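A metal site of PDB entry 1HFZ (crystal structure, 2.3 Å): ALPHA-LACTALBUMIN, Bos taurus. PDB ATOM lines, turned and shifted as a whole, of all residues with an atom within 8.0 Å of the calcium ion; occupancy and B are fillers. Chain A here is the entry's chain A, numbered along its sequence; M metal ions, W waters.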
ATOM      1  N   THR A  39      28.160   8.453  -4.412  1.00  0.00           N
ATOM      2  CA  THR A  39      27.000   8.458  -5.338  1.00  0.00           C
ATOM      3  C   THR A  39      25.628   8.447  -4.680  1.00  0.00           C
ATOM      4  O   THR A  39      24.618   8.686  -5.353  1.00  0.00           O
ATOM      5  CB  THR A  39      27.074   7.295  -6.342  1.00  0.00           C
ATOM      6  OG1 THR A  39      27.448   6.092  -5.655  1.00  0.00           O
ATOM      7  CG2 THR A  39      28.110   7.563  -7.418  1.00  0.00           C
ATOM      8  N   GLY A  52      22.852  12.460  -4.746  1.00  0.00           N
ATOM      9  CA  GLY A  52      23.999  11.962  -5.502  1.00  0.00           C
ATOM     10  C   GLY A  52      25.362  12.625  -5.456  1.00  0.00           C
ATOM     11  O   GLY A  52      25.668  13.472  -4.604  1.00  0.00           O
ATOM     12  N   ILE A  76      13.069  14.156 -14.109  1.00  0.00           N
ATOM     13  CA  ILE A  76      13.466  12.846 -13.664  1.00  0.00           C
ATOM     14  C   ILE A  76      13.204  12.716 -12.193  1.00  0.00           C
ATOM     15  O   ILE A  76      12.917  13.701 -11.517  1.00  0.00           O
ATOM     16  CB  ILE A  76      14.964  12.697 -13.934  1.00  0.00           C
ATOM     17  CG1 ILE A  76      15.441  11.283 -13.684  1.00  0.00           C
ATOM     18  CG2 ILE A  76      15.755  13.685 -13.084  1.00  0.00           C
ATOM     19  CD1 ILE A  76      16.843  11.070 -14.212  1.00  0.00           C
ATOM     20  N   SER A  77      13.229  11.491 -11.697  1.00  0.00           N
ATOM     21  CA  SER A  77      13.026  11.255 -10.286  1.00  0.00           C
ATOM     22  C   SER A  77      14.397  11.376  -9.641  1.00  0.00           C
ATOM     23  O   SER A  77      15.379  10.857 -10.165  1.00  0.00           O
ATOM     24  CB  SER A  77      12.437   9.860 -10.082  1.00  0.00           C
ATOM     25  OG  SER A  77      12.164   9.635  -8.711  1.00  0.00           O
ATOM     26  N   CYS A  78      14.479  12.032  -8.485  1.00  0.00           N
ATOM     27  CA  CYS A  78      15.758  12.228  -7.784  1.00  0.00           C
ATOM     28  C   CYS A  78      16.520  10.961  -7.396  1.00  0.00           C
ATOM     29  O   CYS A  78      17.737  10.997  -7.187  1.00  0.00           O
ATOM     30  CB  CYS A  78      15.568  13.044  -6.499  1.00  0.00           C
ATOM     31  SG  CYS A  78      14.997  14.762  -6.660  1.00  0.00           S
ATOM     32  N   ASP A  79      15.795   9.868  -7.187  1.00  0.00           N
ATOM     33  CA  ASP A  79      16.394   8.602  -6.789  1.00  0.00           C
ATOM     34  C   ASP A  79      17.264   8.006  -7.879  1.00  0.00           C
ATOM     35  O   ASP A  79      18.211   7.274  -7.599  1.00  0.00           O
ATOM     36  CB  ASP A  79      15.325   7.637  -6.304  1.00  0.00           C
ATOM     37  CG  ASP A  79      14.020   7.779  -7.071  1.00  0.00           C
ATOM     38  OD1 ASP A  79      14.068   7.834  -8.326  1.00  0.00           O
ATOM     39  OD2 ASP A  79      12.945   7.852  -6.419  1.00  0.00           O
ATOM     40  N   LYS A  80      17.000   8.387  -9.131  1.00  0.00           N
ATOM     41  CA  LYS A  80      17.810   7.907 -10.234  1.00  0.00           C
ATOM     42  C   LYS A  80      19.224   8.505 -10.174  1.00  0.00           C
ATOM     43  O   LYS A  80      20.110   8.167 -10.975  1.00  0.00           O
ATOM     44  CB  LYS A  80      17.119   8.207 -11.555  1.00  0.00           C
ATOM     45  CG  LYS A  80      15.876   7.309 -11.749  1.00  0.00           C
ATOM     46  CD  LYS A  80      15.455   7.166 -13.200  1.00  0.00           C
ATOM     47  CE  LYS A  80      14.424   8.235 -13.644  1.00  0.00           C
ATOM     48  NZ  LYS A  80      13.048   8.125 -13.026  1.00  0.00           N
ATOM     49  N   PHE A  81      19.429   9.415  -9.234  1.00  0.00           N
ATOM     50  CA  PHE A  81      20.720  10.036  -9.012  1.00  0.00           C
ATOM     51  C   PHE A  81      21.413   9.339  -7.853  1.00  0.00           C
ATOM     52  O   PHE A  81      22.518   9.692  -7.472  1.00  0.00           O
ATOM     53  CB  PHE A  81      20.583  11.525  -8.632  1.00  0.00           C
ATOM     54  CG  PHE A  81      20.034  12.386  -9.711  1.00  0.00           C
ATOM     55  CD1 PHE A  81      20.133  12.008 -11.033  1.00  0.00           C
ATOM     56  CD2 PHE A  81      19.386  13.583  -9.401  1.00  0.00           C
ATOM     57  CE1 PHE A  81      19.629  12.798 -12.044  1.00  0.00           C
ATOM     58  CE2 PHE A  81      18.864  14.397 -10.401  1.00  0.00           C
ATOM     59  CZ  PHE A  81      18.993  13.997 -11.727  1.00  0.00           C
ATOM     60  N   LEU A  82      20.755   8.351  -7.260  1.00  0.00           N
ATOM     61  CA  LEU A  82      21.373   7.667  -6.116  1.00  0.00           C
ATOM     62  C   LEU A  82      21.979   6.327  -6.504  1.00  0.00           C
ATOM     63  O   LEU A  82      22.592   5.647  -5.679  1.00  0.00           O
ATOM     64  CB  LEU A  82      20.366   7.502  -4.987  1.00  0.00           C
ATOM     65  CG  LEU A  82      19.848   8.766  -4.322  1.00  0.00           C
ATOM     66  CD1 LEU A  82      18.651   8.435  -3.462  1.00  0.00           C
ATOM     67  CD2 LEU A  82      20.950   9.383  -3.505  1.00  0.00           C
ATOM     68  N   ASP A  83      21.822   5.955  -7.785  1.00  0.00           N
ATOM     69  CA  ASP A  83      22.357   4.693  -8.252  1.00  0.00           C
ATOM     70  C   ASP A  83      23.783   4.844  -8.697  1.00  0.00           C
ATOM     71  O   ASP A  83      24.341   5.931  -8.619  1.00  0.00           O
ATOM     72  CB  ASP A  83      21.486   4.066  -9.349  1.00  0.00           C
ATOM     73  CG  ASP A  83      21.379   4.936 -10.581  1.00  0.00           C
ATOM     74  OD1 ASP A  83      22.262   5.795 -10.790  1.00  0.00           O
ATOM     75  OD2 ASP A  83      20.402   4.769 -11.352  1.00  0.00           O
ATOM     76  N   ASP A  84      24.319   3.765  -9.269  1.00  0.00           N
ATOM     77  CA  ASP A  84      25.703   3.677  -9.725  1.00  0.00           C
ATOM     78  C   ASP A  84      25.974   4.234 -11.118  1.00  0.00           C
ATOM     79  O   ASP A  84      27.124   4.415 -11.478  1.00  0.00           O
ATOM     80  CB  ASP A  84      26.171   2.218  -9.663  1.00  0.00           C
ATOM     81  CG  ASP A  84      25.172   1.285 -10.295  1.00  0.00           C
ATOM     82  OD1 ASP A  84      24.131   1.003  -9.658  1.00  0.00           O
ATOM     83  OD2 ASP A  84      25.407   0.860 -11.457  1.00  0.00           O
ATOM     84  N   ASP A  85      24.942   4.456 -11.905  1.00  0.00           N
ATOM     85  CA  ASP A  85      25.093   5.014 -13.248  1.00  0.00           C
ATOM     86  C   ASP A  85      24.958   6.552 -13.221  1.00  0.00           C
ATOM     87  O   ASP A  85      23.887   7.096 -12.877  1.00  0.00           O
ATOM     88  CB  ASP A  85      24.033   4.419 -14.170  1.00  0.00           C
ATOM     89  CG  ASP A  85      24.253   4.790 -15.614  1.00  0.00           C
ATOM     90  OD1 ASP A  85      25.353   5.279 -15.964  1.00  0.00           O
ATOM     91  OD2 ASP A  85      23.323   4.585 -16.430  1.00  0.00           O
ATOM     92  N   LEU A  86      26.020   7.249 -13.616  1.00  0.00           N
ATOM     93  CA  LEU A  86      26.047   8.724 -13.611  1.00  0.00           C
ATOM     94  C   LEU A  86      25.671   9.305 -14.960  1.00  0.00           C
ATOM     95  O   LEU A  86      25.780  10.503 -15.185  1.00  0.00           O
ATOM     96  CB  LEU A  86      27.438   9.252 -13.183  1.00  0.00           C
ATOM     97  CG  LEU A  86      28.072   8.790 -11.853  1.00  0.00           C
ATOM     98  CD1 LEU A  86      29.388   9.462 -11.630  1.00  0.00           C
ATOM     99  CD2 LEU A  86      27.163   9.073 -10.702  1.00  0.00           C
ATOM    100  N   THR A  87      25.172   8.474 -15.853  1.00  0.00           N
ATOM    101  CA  THR A  87      24.778   8.905 -17.193  1.00  0.00           C
ATOM    102  C   THR A  87      23.684   9.967 -17.159  1.00  0.00           C
ATOM    103  O   THR A  87      23.791  11.022 -17.827  1.00  0.00           O
ATOM    104  CB  THR A  87      24.343   7.679 -18.043  1.00  0.00           C
ATOM    105  OG1 THR A  87      25.488   6.852 -18.306  1.00  0.00           O
ATOM    106  CG2 THR A  87      23.709   8.117 -19.367  1.00  0.00           C
ATOM    107  N   ASP A  88      22.619   9.700 -16.415  1.00  0.00           N
ATOM    108  CA  ASP A  88      21.569  10.676 -16.337  1.00  0.00           C
ATOM    109  C   ASP A  88      21.928  11.850 -15.429  1.00  0.00           C
ATOM    110  O   ASP A  88      21.475  12.961 -15.658  1.00  0.00           O
ATOM    111  CB  ASP A  88      20.220  10.033 -15.988  1.00  0.00           C
ATOM    112  CG  ASP A  88      20.283   9.107 -14.796  1.00  0.00           C
ATOM    113  OD1 ASP A  88      21.320   9.004 -14.116  1.00  0.00           O
ATOM    114  OD2 ASP A  88      19.236   8.485 -14.531  1.00  0.00           O
ATOM    115  N   ASP A  89      22.796  11.608 -14.453  1.00  0.00           N
ATOM    116  CA  ASP A  89      23.210  12.685 -13.561  1.00  0.00           C
ATOM    117  C   ASP A  89      23.874  13.719 -14.456  1.00  0.00           C
ATOM    118  O   ASP A  89      23.605  14.910 -14.356  1.00  0.00           O
ATOM    119  CB  ASP A  89      24.249  12.185 -12.562  1.00  0.00           C
ATOM    120  CG  ASP A  89      23.730  11.105 -11.690  1.00  0.00           C
ATOM    121  OD1 ASP A  89      23.161  10.132 -12.245  1.00  0.00           O
ATOM    122  OD2 ASP A  89      23.907  11.200 -10.447  1.00  0.00           O
ATOM    123  N   ILE A  90      24.743  13.234 -15.333  1.00  0.00           N
ATOM    124  CA  ILE A  90      25.449  14.061 -16.292  1.00  0.00           C
ATOM    125  C   ILE A  90      24.444  14.808 -17.170  1.00  0.00           C
ATOM    126  O   ILE A  90      24.690  15.959 -17.534  1.00  0.00           O
ATOM    127  CB  ILE A  90      26.397  13.208 -17.201  1.00  0.00           C
ATOM    128  CG1 ILE A  90      27.810  13.114 -16.631  1.00  0.00           C
ATOM    129  CG2 ILE A  90      26.461  13.787 -18.597  1.00  0.00           C
ATOM    130  CD1 ILE A  90      27.919  12.398 -15.328  1.00  0.00           C
HETATM  131 CA    CA M   1      21.967   7.850 -12.002  1.00  0.00          CA
HETATM  132  O   HOH W   1      20.256   6.130 -13.344  1.00  0.00           O
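The side-chain carboxylate (OD1) of Asp 85 lies within hydrogen-bond range of the side-chain hydroxyl (OG1) of Thr 87, at 2.8 Å.
Merely in contact with the calcium ion: Phe 81 (3.9 Å).
Within 4 Å of the calcium ion: Lys 80, Phe 81, Asp 83, Asp 85, Asp 88 and Asp 89.
The nearest printed residue that does not touch the calcium ion is Leu 86 (4.4 Å).
Water W1 lies within hydrogen-bond range of OD2 of Asp 83 (2.4 Å) and OD2 of Asp 88 (2.8 Å).
The calcium ion is bound by O of Lys 80 (2.1 Å), O of Asp 85 (2.2 Å), OD1 of Asp 83 (2.4 Å), OD1 of Asp 88 (2.5 Å), OD1 of Asp 89 (2.6 Å) and water W1 (2.8 Å).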
